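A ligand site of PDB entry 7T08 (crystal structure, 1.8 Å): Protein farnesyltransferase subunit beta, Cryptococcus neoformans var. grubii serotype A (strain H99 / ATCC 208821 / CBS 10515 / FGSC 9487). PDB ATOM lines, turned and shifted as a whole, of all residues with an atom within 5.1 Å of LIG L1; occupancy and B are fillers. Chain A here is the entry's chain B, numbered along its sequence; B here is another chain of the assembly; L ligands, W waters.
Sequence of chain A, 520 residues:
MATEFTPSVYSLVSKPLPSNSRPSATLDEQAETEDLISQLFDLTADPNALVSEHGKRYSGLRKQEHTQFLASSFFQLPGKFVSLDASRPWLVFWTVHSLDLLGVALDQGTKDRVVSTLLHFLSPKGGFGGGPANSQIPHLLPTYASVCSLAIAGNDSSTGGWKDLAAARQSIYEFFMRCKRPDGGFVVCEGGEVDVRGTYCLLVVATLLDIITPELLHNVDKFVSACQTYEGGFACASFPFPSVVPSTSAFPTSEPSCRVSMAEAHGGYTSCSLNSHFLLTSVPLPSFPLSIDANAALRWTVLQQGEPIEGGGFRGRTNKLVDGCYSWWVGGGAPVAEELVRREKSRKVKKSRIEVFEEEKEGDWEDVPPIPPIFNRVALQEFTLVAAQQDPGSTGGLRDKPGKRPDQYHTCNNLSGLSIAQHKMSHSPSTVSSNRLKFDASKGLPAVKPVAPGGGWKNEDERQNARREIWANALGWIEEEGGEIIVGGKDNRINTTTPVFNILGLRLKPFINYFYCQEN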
ATOM      1  N   TRP A  90     -13.193 -33.105 -17.159  1.00  0.00           N
ATOM      2  CA  TRP A  90     -12.887 -32.212 -16.035  1.00  0.00           C
ATOM      3  C   TRP A  90     -13.616 -32.662 -14.764  1.00  0.00           C
ATOM      4  O   TRP A  90     -13.053 -32.580 -13.665  1.00  0.00           O
ATOM      5  CB  TRP A  90     -13.285 -30.772 -16.380  1.00  0.00           C
ATOM      6  CG  TRP A  90     -12.356 -30.169 -17.384  1.00  0.00           C
ATOM      7  CD1 TRP A  90     -12.606 -29.950 -18.720  1.00  0.00           C
ATOM      8  CD2 TRP A  90     -11.013 -29.731 -17.149  1.00  0.00           C
ATOM      9  NE1 TRP A  90     -11.498 -29.391 -19.323  1.00  0.00           N
ATOM     10  CE2 TRP A  90     -10.506 -29.250 -18.377  1.00  0.00           C
ATOM     11  CE3 TRP A  90     -10.183 -29.700 -16.021  1.00  0.00           C
ATOM     12  CZ2 TRP A  90      -9.215 -28.735 -18.511  1.00  0.00           C
ATOM     13  CZ3 TRP A  90      -8.906 -29.189 -16.158  1.00  0.00           C
ATOM     14  CH2 TRP A  90      -8.425 -28.715 -17.390  1.00  0.00           C
ATOM     15  N   LEU A 141      -8.478 -29.190 -24.088  1.00  0.00           N
ATOM     16  CA  LEU A 141      -8.645 -29.089 -22.640  1.00  0.00           C
ATOM     17  C   LEU A 141      -9.088 -30.422 -22.046  1.00  0.00           C
ATOM     18  O   LEU A 141      -8.499 -30.864 -21.050  1.00  0.00           O
ATOM     19  CB  LEU A 141      -9.610 -27.949 -22.300  1.00  0.00           C
ATOM     20  CG  LEU A 141      -8.986 -26.574 -22.029  1.00  0.00           C
ATOM     21  CD1 LEU A 141      -8.172 -26.096 -23.228  1.00  0.00           C
ATOM     22  CD2 LEU A 141     -10.071 -25.551 -21.677  1.00  0.00           C
ATOM     23  N   ARG A 197      -4.628 -21.260 -22.578  1.00  0.00           N
ATOM     24  CA  ARG A 197      -5.149 -22.503 -22.007  1.00  0.00           C
ATOM     25  C   ARG A 197      -4.849 -23.672 -22.923  1.00  0.00           C
ATOM     26  O   ARG A 197      -4.455 -24.758 -22.467  1.00  0.00           O
ATOM     27  CB  ARG A 197      -6.676 -22.426 -21.761  1.00  0.00           C
ATOM     28  CG  ARG A 197      -7.169 -21.381 -20.726  1.00  0.00           C
ATOM     29  CD  ARG A 197      -8.700 -21.213 -20.800  1.00  0.00           C
ATOM     30  NE  ARG A 197      -9.119 -21.009 -22.205  1.00  0.00           N
ATOM     31  CZ  ARG A 197     -10.212 -21.548 -22.746  1.00  0.00           C
ATOM     32  NH1 ARG A 197     -11.040 -22.296 -22.010  1.00  0.00           N
ATOM     33  NH2 ARG A 197     -10.467 -21.365 -24.034  1.00  0.00           N
ATOM     34  N   TYR A 200      -1.021 -24.481 -22.752  1.00  0.00           N
ATOM     35  CA  TYR A 200      -0.671 -25.197 -21.527  1.00  0.00           C
ATOM     36  C   TYR A 200      -1.106 -26.648 -21.599  1.00  0.00           C
ATOM     37  O   TYR A 200      -0.319 -27.565 -21.342  1.00  0.00           O
ATOM     38  CB  TYR A 200      -1.306 -24.485 -20.308  1.00  0.00           C
ATOM     39  CG  TYR A 200      -1.294 -25.368 -19.057  1.00  0.00           C
ATOM     40  CD1 TYR A 200      -0.129 -25.544 -18.323  1.00  0.00           C
ATOM     41  CD2 TYR A 200      -2.445 -26.039 -18.657  1.00  0.00           C
ATOM     42  CE1 TYR A 200      -0.111 -26.377 -17.190  1.00  0.00           C
ATOM     43  CE2 TYR A 200      -2.436 -26.869 -17.521  1.00  0.00           C
ATOM     44  CZ  TYR A 200      -1.268 -27.018 -16.803  1.00  0.00           C
ATOM     45  OH  TYR A 200      -1.256 -27.845 -15.690  1.00  0.00           O
ATOM     46  N   CYS A 201      -2.380 -26.890 -21.932  1.00  0.00           N
ATOM     47  CA  CYS A 201      -2.875 -28.268 -21.935  1.00  0.00           C
ATOM     48  C   CYS A 201      -2.107 -29.110 -22.932  1.00  0.00           C
ATOM     49  O   CYS A 201      -1.783 -30.281 -22.652  1.00  0.00           O
ATOM     50  CB  CYS A 201      -4.379 -28.285 -22.255  1.00  0.00           C
ATOM     51  SG  CYS A 201      -5.420 -27.634 -20.939  1.00  0.00           S
ATOM     52  N   HIS A 266      -4.579 -12.057 -15.896  1.00  0.00           N
ATOM     53  CA  HIS A 266      -5.496 -12.849 -15.086  1.00  0.00           C
ATOM     54  C   HIS A 266      -4.771 -14.044 -14.496  1.00  0.00           C
ATOM     55  O   HIS A 266      -3.869 -14.627 -15.115  1.00  0.00           O
ATOM     56  CB  HIS A 266      -6.701 -13.354 -15.910  1.00  0.00           C
ATOM     57  CG  HIS A 266      -7.871 -13.731 -15.063  1.00  0.00           C
ATOM     58  ND1 HIS A 266      -7.950 -14.926 -14.375  1.00  0.00           N
ATOM     59  CD2 HIS A 266      -8.986 -13.032 -14.741  1.00  0.00           C
ATOM     60  CE1 HIS A 266      -9.075 -14.957 -13.680  1.00  0.00           C
ATOM     61  NE2 HIS A 266      -9.721 -13.815 -13.882  1.00  0.00           N
ATOM     62  N   GLY A 268      -5.785 -17.103 -14.113  1.00  0.00           N
ATOM     63  CA  GLY A 268      -5.911 -18.322 -14.909  1.00  0.00           C
ATOM     64  C   GLY A 268      -4.933 -18.356 -16.078  1.00  0.00           C
ATOM     65  O   GLY A 268      -4.287 -19.386 -16.350  1.00  0.00           O
ATOM     66  N   TYR A 269      -4.796 -17.234 -16.781  1.00  0.00           N
ATOM     67  CA  TYR A 269      -3.894 -17.182 -17.935  1.00  0.00           C
ATOM     68  C   TYR A 269      -2.444 -16.978 -17.527  1.00  0.00           C
ATOM     69  O   TYR A 269      -1.543 -17.369 -18.270  1.00  0.00           O
ATOM     70  CB  TYR A 269      -4.358 -16.058 -18.860  1.00  0.00           C
ATOM     71  CG  TYR A 269      -5.743 -16.269 -19.439  1.00  0.00           C
ATOM     72  CD1 TYR A 269      -6.082 -17.448 -20.065  1.00  0.00           C
ATOM     73  CD2 TYR A 269      -6.713 -15.281 -19.339  1.00  0.00           C
ATOM     74  CE1 TYR A 269      -7.347 -17.662 -20.601  1.00  0.00           C
ATOM     75  CE2 TYR A 269      -7.986 -15.474 -19.857  1.00  0.00           C
ATOM     76  CZ  TYR A 269      -8.294 -16.656 -20.488  1.00  0.00           C
ATOM     77  OH  TYR A 269      -9.555 -16.839 -21.011  1.00  0.00           O
ATOM     78  N   CYS A 272      -1.302 -20.521 -16.779  1.00  0.00           N
ATOM     79  CA  CYS A 272      -1.061 -21.273 -18.005  1.00  0.00           C
ATOM     80  C   CYS A 272       0.212 -20.787 -18.697  1.00  0.00           C
ATOM     81  O   CYS A 272       0.978 -21.607 -19.235  1.00  0.00           O
ATOM     82  CB  CYS A 272      -2.274 -21.162 -18.941  1.00  0.00           C
ATOM     83  SG  CYS A 272      -3.735 -22.108 -18.373  1.00  0.00           S
ATOM     84  N   GLY A 316      -8.176 -12.903  -8.789  1.00  0.00           N
ATOM     85  CA  GLY A 316      -7.734 -13.314 -10.116  1.00  0.00           C
ATOM     86  C   GLY A 316      -7.227 -12.159 -10.978  1.00  0.00           C
ATOM     87  O   GLY A 316      -6.517 -12.388 -11.951  1.00  0.00           O
ATOM     88  N   ARG A 317      -7.601 -10.930 -10.643  1.00  0.00           N
ATOM     89  CA  ARG A 317      -7.084  -9.758 -11.356  1.00  0.00           C
ATOM     90  C   ARG A 317      -7.291  -8.522 -10.494  1.00  0.00           C
ATOM     91  O   ARG A 317      -8.113  -8.519  -9.564  1.00  0.00           O
ATOM     92  CB  ARG A 317      -7.741  -9.590 -12.748  1.00  0.00           C
ATOM     93  CG  ARG A 317      -9.236  -9.921 -12.838  1.00  0.00           C
ATOM     94  CD  ARG A 317      -9.835  -9.599 -14.232  1.00  0.00           C
ATOM     95  NE  ARG A 317     -11.151 -10.233 -14.361  1.00  0.00           N
ATOM     96  CZ  ARG A 317     -12.118  -9.826 -15.187  1.00  0.00           C
ATOM     97  NH1 ARG A 317     -11.920  -8.784 -16.005  1.00  0.00           N
ATOM     98  NH2 ARG A 317     -13.282 -10.460 -15.194  1.00  0.00           N
ATOM     99  N   LYS A 320     -10.693  -6.831  -8.613  1.00  0.00           N
ATOM    100  CA  LYS A 320     -11.791  -7.775  -8.536  1.00  0.00           C
ATOM    101  C   LYS A 320     -11.698  -8.512  -7.191  1.00  0.00           C
ATOM    102  O   LYS A 320     -10.993  -8.061  -6.284  1.00  0.00           O
ATOM    103  CB  LYS A 320     -11.799  -8.709  -9.758  1.00  0.00           C
ATOM    104  CG  LYS A 320     -12.089  -7.913 -11.077  1.00  0.00           C
ATOM    105  CD  LYS A 320     -13.005  -8.687 -12.039  1.00  0.00           C
ATOM    106  CE  LYS A 320     -14.468  -8.660 -11.589  1.00  0.00           C
ATOM    107  NZ  LYS A 320     -15.287  -9.724 -12.266  1.00  0.00           N
ATOM    108  N   LEU A 321     -12.466  -9.585  -7.025  1.00  0.00           N
ATOM    109  CA  LEU A 321     -12.666 -10.172  -5.699  1.00  0.00           C
ATOM    110  C   LEU A 321     -11.815 -11.418  -5.457  1.00  0.00           C
ATOM    111  O   LEU A 321     -11.474 -12.166  -6.381  1.00  0.00           O
ATOM    112  CB  LEU A 321     -14.147 -10.511  -5.490  1.00  0.00           C
ATOM    113  CG  LEU A 321     -15.184  -9.389  -5.708  1.00  0.00           C
ATOM    114  CD1 LEU A 321     -16.585  -9.958  -5.627  1.00  0.00           C
ATOM    115  CD2 LEU A 321     -14.999  -8.235  -4.706  1.00  0.00           C
ATOM    116  N   ASP A 323     -11.125 -15.236  -4.331  1.00  0.00           N
ATOM    117  CA  ASP A 323     -11.874 -16.436  -4.706  1.00  0.00           C
ATOM    118  C   ASP A 323     -10.966 -17.636  -4.480  1.00  0.00           C
ATOM    119  O   ASP A 323      -9.807 -17.632  -4.921  1.00  0.00           O
ATOM    120  CB  ASP A 323     -12.338 -16.327  -6.190  1.00  0.00           C
ATOM    121  CG  ASP A 323     -12.954 -17.618  -6.748  1.00  0.00           C
ATOM    122  OD1 ASP A 323     -12.851 -18.708  -6.128  1.00  0.00           O
ATOM    123  OD2 ASP A 323     -13.541 -17.549  -7.846  1.00  0.00           O
ATOM    124  N   TYR A 326      -8.382 -19.386  -6.982  1.00  0.00           N
ATOM    125  CA  TYR A 326      -7.101 -18.777  -7.313  1.00  0.00           C
ATOM    126  C   TYR A 326      -5.999 -19.161  -6.343  1.00  0.00           C
ATOM    127  O   TYR A 326      -4.834 -18.792  -6.570  1.00  0.00           O
ATOM    128  CB  TYR A 326      -7.260 -17.236  -7.412  1.00  0.00           C
ATOM    129  CG  TYR A 326      -8.287 -16.875  -8.488  1.00  0.00           C
ATOM    130  CD1 TYR A 326      -8.195 -17.415  -9.770  1.00  0.00           C
ATOM    131  CD2 TYR A 326      -9.357 -16.039  -8.208  1.00  0.00           C
ATOM    132  CE1 TYR A 326      -9.144 -17.133 -10.747  1.00  0.00           C
ATOM    133  CE2 TYR A 326     -10.320 -15.724  -9.195  1.00  0.00           C
ATOM    134  CZ  TYR A 326     -10.195 -16.287 -10.460  1.00  0.00           C
ATOM    135  OH  TYR A 326     -11.112 -16.007 -11.441  1.00  0.00           O
ATOM    136  N   TRP A 329      -4.549 -21.238  -9.090  1.00  0.00           N
ATOM    137  CA  TRP A 329      -4.132 -20.555 -10.307  1.00  0.00           C
ATOM    138  C   TRP A 329      -3.065 -19.506 -10.021  1.00  0.00           C
ATOM    139  O   TRP A 329      -2.089 -19.383 -10.771  1.00  0.00           O
ATOM    140  CB  TRP A 329      -5.333 -19.926 -11.040  1.00  0.00           C
ATOM    141  CG  TRP A 329      -6.392 -20.923 -11.414  1.00  0.00           C
ATOM    142  CD1 TRP A 329      -7.688 -20.954 -10.947  1.00  0.00           C
ATOM    143  CD2 TRP A 329      -6.255 -22.056 -12.287  1.00  0.00           C
ATOM    144  NE1 TRP A 329      -8.359 -22.039 -11.493  1.00  0.00           N
ATOM    145  CE2 TRP A 329      -7.496 -22.721 -12.316  1.00  0.00           C
ATOM    146  CE3 TRP A 329      -5.188 -22.562 -13.051  1.00  0.00           C
ATOM    147  CZ2 TRP A 329      -7.715 -23.883 -13.083  1.00  0.00           C
ATOM    148  CZ3 TRP A 329      -5.407 -23.718 -13.825  1.00  0.00           C
ATOM    149  CH2 TRP A 329      -6.651 -24.363 -13.822  1.00  0.00           C
ATOM    150  N   TYR A 409     -15.153 -28.030  -9.135  1.00  0.00           N
ATOM    151  CA  TYR A 409     -14.045 -27.224  -9.627  1.00  0.00           C
ATOM    152  C   TYR A 409     -13.387 -26.448  -8.484  1.00  0.00           C
ATOM    153  O   TYR A 409     -12.153 -26.392  -8.391  1.00  0.00           O
ATOM    154  CB  TYR A 409     -14.551 -26.285 -10.738  1.00  0.00           C
ATOM    155  CG  TYR A 409     -13.682 -25.069 -10.985  1.00  0.00           C
ATOM    156  CD1 TYR A 409     -12.616 -25.103 -11.906  1.00  0.00           C
ATOM    157  CD2 TYR A 409     -13.917 -23.872 -10.301  1.00  0.00           C
ATOM    158  CE1 TYR A 409     -11.811 -23.967 -12.126  1.00  0.00           C
ATOM    159  CE2 TYR A 409     -13.120 -22.739 -10.509  1.00  0.00           C
ATOM    160  CZ  TYR A 409     -12.076 -22.794 -11.407  1.00  0.00           C
ATOM    161  OH  TYR A 409     -11.299 -21.664 -11.577  1.00  0.00           O
ATOM    162  N   TYR B 123     -17.361 -19.413 -23.644  1.00  0.00           N
ATOM    163  CA  TYR B 123     -16.288 -19.212 -24.625  1.00  0.00           C
ATOM    164  C   TYR B 123     -16.780 -19.495 -26.040  1.00  0.00           C
ATOM    165  O   TYR B 123     -16.351 -18.840 -27.001  1.00  0.00           O
ATOM    166  CB  TYR B 123     -15.092 -20.128 -24.344  1.00  0.00           C
ATOM    167  CG  TYR B 123     -14.124 -19.719 -23.254  1.00  0.00           C
ATOM    168  CD1 TYR B 123     -12.998 -18.928 -23.547  1.00  0.00           C
ATOM    169  CD2 TYR B 123     -14.278 -20.183 -21.957  1.00  0.00           C
ATOM    170  CE1 TYR B 123     -12.076 -18.607 -22.544  1.00  0.00           C
ATOM    171  CE2 TYR B 123     -13.374 -19.849 -20.955  1.00  0.00           C
ATOM    172  CZ  TYR B 123     -12.270 -19.081 -21.253  1.00  0.00           C
ATOM    173  OH  TYR B 123     -11.365 -18.783 -20.243  1.00  0.00           O
ATOM    174  N   LYS B 157     -16.779  -5.582 -16.543  1.00  0.00           N
ATOM    175  CA  LYS B 157     -15.465  -6.222 -16.482  1.00  0.00           C
ATOM    176  C   LYS B 157     -15.452  -7.588 -17.164  1.00  0.00           C
ATOM    177  O   LYS B 157     -14.489  -8.341 -16.990  1.00  0.00           O
ATOM    178  CB  LYS B 157     -14.993  -6.368 -15.030  1.00  0.00           C
ATOM    179  CG  LYS B 157     -14.921  -5.027 -14.283  1.00  0.00           C
ATOM    180  CD  LYS B 157     -14.376  -5.157 -12.862  1.00  0.00           C
ATOM    181  CE  LYS B 157     -14.210  -3.782 -12.198  1.00  0.00           C
ATOM    182  NZ  LYS B 157     -13.544  -3.901 -10.856  1.00  0.00           N
ATOM    183  N   TYR B 159     -14.524 -10.459 -19.078  1.00  0.00           N
ATOM    184  CA  TYR B 159     -13.212 -10.669 -19.678  1.00  0.00           C
ATOM    185  C   TYR B 159     -13.327 -11.006 -21.154  1.00  0.00           C
ATOM    186  O   TYR B 159     -12.556 -10.493 -21.985  1.00  0.00           O
ATOM    187  CB  TYR B 159     -12.449 -11.768 -18.913  1.00  0.00           C
ATOM    188  CG  TYR B 159     -10.967 -11.804 -19.279  1.00  0.00           C
ATOM    189  CD1 TYR B 159     -10.532 -12.387 -20.464  1.00  0.00           C
ATOM    190  CD2 TYR B 159     -10.021 -11.221 -18.434  1.00  0.00           C
ATOM    191  CE1 TYR B 159      -9.178 -12.387 -20.816  1.00  0.00           C
ATOM    192  CE2 TYR B 159      -8.666 -11.241 -18.764  1.00  0.00           C
ATOM    193  CZ  TYR B 159      -8.253 -11.824 -19.947  1.00  0.00           C
ATOM    194  OH  TYR B 159      -6.912 -11.817 -20.279  1.00  0.00           O
ATOM    195  N   HIS B 160     -14.297 -11.865 -21.519  1.00  0.00           N
ATOM    196  CA  HIS B 160     -14.493 -12.219 -22.924  1.00  0.00           C
ATOM    197  C   HIS B 160     -14.782 -10.996 -23.761  1.00  0.00           C
ATOM    198  O   HIS B 160     -14.319 -10.901 -24.912  1.00  0.00           O
ATOM    199  CB  HIS B 160     -15.649 -13.205 -23.067  1.00  0.00           C
ATOM    200  CG  HIS B 160     -15.520 -14.420 -22.211  1.00  0.00           C
ATOM    201  ND1 HIS B 160     -14.515 -15.355 -22.387  1.00  0.00           N
ATOM    202  CD2 HIS B 160     -16.279 -14.871 -21.180  1.00  0.00           C
ATOM    203  CE1 HIS B 160     -14.650 -16.315 -21.488  1.00  0.00           C
ATOM    204  NE2 HIS B 160     -15.711 -16.052 -20.739  1.00  0.00           N
HETATM  205  C1  LIG L   1     -12.750 -14.454 -15.826  1.00  0.00           C
HETATM  206  O1  LIG L   1     -13.927 -14.987 -15.249  1.00  0.00           O
HETATM  207  C2  LIG L   1     -11.739 -15.584 -16.093  1.00  0.00           C
HETATM  208  C3  LIG L   1     -11.406 -16.048 -17.299  1.00  0.00           C
HETATM  209  C4  LIG L   1     -12.023 -15.482 -18.597  1.00  0.00           C
HETATM  210  C5  LIG L   1     -10.388 -17.186 -17.454  1.00  0.00           C
HETATM  211  C6  LIG L   1      -9.911 -17.824 -16.129  1.00  0.00           C
HETATM  212  C7  LIG L   1      -9.126 -19.119 -16.432  1.00  0.00           C
HETATM  213  C8  LIG L   1      -8.809 -19.988 -15.458  1.00  0.00           C
HETATM  214  C9  LIG L   1      -9.188 -19.698 -14.002  1.00  0.00           C
HETATM  215  C10 LIG L   1      -8.032 -21.292 -15.689  1.00  0.00           C
HETATM  216  C11 LIG L   1      -7.773 -21.722 -17.140  1.00  0.00           C
HETATM  217  C12 LIG L   1      -6.802 -22.926 -17.123  1.00  0.00           C
HETATM  218  C13 LIG L   1      -6.986 -24.091 -17.774  1.00  0.00           C
HETATM  219  C14 LIG L   1      -5.916 -25.186 -17.669  1.00  0.00           C
HETATM  220  C15 LIG L   1      -8.214 -24.363 -18.645  1.00  0.00           C
HETATM  221  P1  LIG L   1     -14.788 -14.149 -14.115  1.00  0.00           P
HETATM  222  O2  LIG L   1     -15.015 -12.711 -14.514  1.00  0.00           O
HETATM  223  O3  LIG L   1     -16.067 -14.909 -13.891  1.00  0.00           O
HETATM  224  O4  LIG L   1     -13.957 -14.205 -12.704  1.00  0.00           O
HETATM  225  P2  LIG L   1     -13.052 -13.044 -11.988  1.00  0.00           P
HETATM  226  O5  LIG L   1     -14.006 -11.982 -11.491  1.00  0.00           O
HETATM  227  O6  LIG L   1     -12.030 -12.509 -12.952  1.00  0.00           O
HETATM  228  O7  LIG L   1     -12.405 -13.787 -10.821  1.00  0.00           O
HETATM  229  C1  LG2 L   2     -14.834 -26.312 -17.745  1.00  0.00           C
HETATM  230  C2  LG2 L   2     -16.383 -20.953 -15.465  1.00  0.00           C
HETATM  231  C3  LG2 L   2     -15.393 -19.456 -12.352  1.00  0.00           C
HETATM  232  C4  LG2 L   2     -18.457 -26.187 -11.662  1.00  0.00           C
HETATM  233  C5  LG2 L   2     -18.538 -24.858 -12.448  1.00  0.00           C
HETATM  234  C6  LG2 L   2     -17.190 -24.119 -12.509  1.00  0.00           C
HETATM  235  C7  LG2 L   2     -17.256 -22.834 -13.415  1.00  0.00           C
HETATM  236  C8  LG2 L   2     -15.812 -22.107 -13.507  1.00  0.00           C
HETATM  237  C9  LG2 L   2     -14.869 -23.078 -14.176  1.00  0.00           C
HETATM  238  C10 LG2 L   2     -14.517 -24.364 -16.387  1.00  0.00           C
HETATM  239  C11 LG2 L   2     -15.374 -25.214 -17.074  1.00  0.00           C
HETATM  240  C12 LG2 L   2     -13.471 -26.552 -17.709  1.00  0.00           C
HETATM  241  C13 LG2 L   2     -12.608 -25.708 -17.001  1.00  0.00           C
HETATM  242  C14 LG2 L   2     -10.424 -25.491 -15.969  1.00  0.00           C
HETATM  243  C15 LG2 L   2     -13.149 -24.603 -16.337  1.00  0.00           C
HETATM  244  C16 LG2 L   2     -15.829 -22.152 -16.347  1.00  0.00           C
HETATM  245  C17 LG2 L   2     -16.369 -19.886 -13.499  1.00  0.00           C
HETATM  246  C18 LG2 L   2     -15.460 -19.875 -11.021  1.00  0.00           C
HETATM  247  C19 LG2 L   2     -13.756 -18.538 -11.235  1.00  0.00           C
HETATM  248  C20 LG2 L   2     -13.868 -17.906 -13.633  1.00  0.00           C
HETATM  249  C21 LG2 L   2     -13.365 -18.828 -14.788  1.00  0.00           C
HETATM  250  C22 LG2 L   2     -13.650 -18.512 -16.103  1.00  0.00           C
HETATM  251  C23 LG2 L   2     -13.185 -19.330 -17.137  1.00  0.00           C
HETATM  252  C24 LG2 L   2     -12.425 -20.464 -16.829  1.00  0.00           C
HETATM  253  C25 LG2 L   2     -11.901 -21.385 -17.931  1.00  0.00           C
HETATM  254  C26 LG2 L   2     -12.144 -20.763 -15.512  1.00  0.00           C
HETATM  255  C27 LG2 L   2     -12.605 -19.955 -14.487  1.00  0.00           C
HETATM  256  F1  LG2 L   2     -10.998 -25.729 -14.763  1.00  0.00           F
HETATM  257  F2  LG2 L   2      -9.213 -26.110 -16.041  1.00  0.00           F
HETATM  258  F3  LG2 L   2     -10.223 -24.147 -16.067  1.00  0.00           F
HETATM  259  F4  LG2 L   2     -11.411 -21.867 -15.216  1.00  0.00           F
HETATM  260  N1  LG2 L   2     -15.071 -23.192 -15.650  1.00  0.00           N
HETATM  261  N2  LG2 L   2     -15.840 -20.870 -14.191  1.00  0.00           N
HETATM  262  N3  LG2 L   2     -14.451 -19.287 -10.363  1.00  0.00           N
HETATM  263  N4  LG2 L   2     -14.330 -18.637 -12.428  1.00  0.00           N
HETATM  264  N5  LG2 L   2     -11.494 -22.085 -18.737  1.00  0.00           N
HETATM  265  O1  LG2 L   2     -11.230 -25.988 -17.001  1.00  0.00           O
HETATM  266  O2  LG2 L   2     -16.017 -22.214 -17.522  1.00  0.00           O
HETATM  267  O   HOH W   1     -16.278 -15.992 -11.280  1.00  0.00           O
HETATM  268  O   HOH W   2     -16.405 -10.034 -14.845  1.00  0.00           O
HETATM  269  O   HOH W   3     -10.950 -12.208  -9.097  1.00  0.00           O
HETATM  270  O   HOH W   4     -14.216 -15.295  -9.295  1.00  0.00           O
HETATM  271  O   HOH W   5     -16.603 -12.740 -11.143  1.00  0.00           O
HETATM  272  O   HOH W   6     -18.360 -13.543 -13.403  1.00  0.00           O
HETATM  273  O   HOH W   7     -16.953 -16.820 -15.735  1.00  0.00           O
HETATM  274  O   HOH W   8     -14.243 -11.184  -8.878  1.00  0.00           O
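NZ of Lys 320 lies within salt-bridge range of O5 of LIG L1, at 2.7 Å. NE2 of His 266 is in hydrogen-bond range of O6 of LIG L1 (2.8 Å). A nitrogen (N5) of LG2 L2 is in hydrogen-bond range of the guanidinium group (NH1) of Arg 197, at 3.3 Å. An oxygen (O6) of LIG L1 is in salt-bridge range of the guanidinium group (NE) of Arg 317 (2.8 Å). O7 of LIG L1 lies within hydrogen-bond range of OH of Tyr 326 (2.6 Å).
Residues that only touch LIG L1: Tyr 123 of chain B, Gly 268, Cys 272, Trp 329, Arg 197, Tyr 269, Tyr 200, Leu 141, Tyr 159 of chain B, Tyr 409 and His 160 of chain B. Hydrophobic or aromatic side chains within 4 Å of LIG L1: Leu 141, Tyr 200, His 266, Tyr 269, Tyr 326, Trp 329, Tyr 159 of chain B and His 160 of chain B. 15 residues have an atom within 4 Å of LIG L1: Leu 141, Arg 197, Tyr 200, His 266, Gly 268, Tyr 269, Cys 272, Arg 317, Lys 320, Tyr 326, Trp 329, Tyr 409, Tyr 123 of chain B, Tyr 159 of chain B and His 160 of chain B. The nearest printed residue that does not touch LIG L1 is Cys 201 (4.1 Å).
Water W5 lies within hydrogen-bond range of O5 of LIG L1 and NZ of Lys 320. Water W8 lies within hydrogen-bond range of an oxygen (O5) of LIG L1 and the backbone NH (N) of Leu 321. Water W3 lies within hydrogen-bond range of O7 of LIG L1 (2.8 Å), O of Leu 321 (2.8 Å) and N of Gly 316 (2.9 Å). Water W2 lies within hydrogen-bond range of NZ of Lys 320 (2.8 Å), O2 of LIG L1 (3.0 Å), NH2 of Arg 317 (3.2 Å) and O of Lys 157 of chain B (3.3 Å).
The indole nitrogen (NE1) of Trp 329 lies within hydrogen-bond range of the side-chain hydroxyl (OH) of Tyr 409, 3.0 Å away. The side-chain sulfur (SG) of Cys 272 is in hydrogen-bond range of the backbone carbonyl oxygen (O) of Gly 268, 3.4 Å away. NH1 of Arg 317 lies within hydrogen-bond range of O of Lys 157 of chain B, at 2.8 Å. O of Arg 197 sits at hydrogen-bond distance from SG of Cys 201. OH of Tyr 123 of chain B sits at hydrogen-bond distance from OH of Tyr 269 (2.8 Å). A ring nitrogen (ND1) of His 266 is in hydrogen-bond range of the backbone NH (N) of Gly 268.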
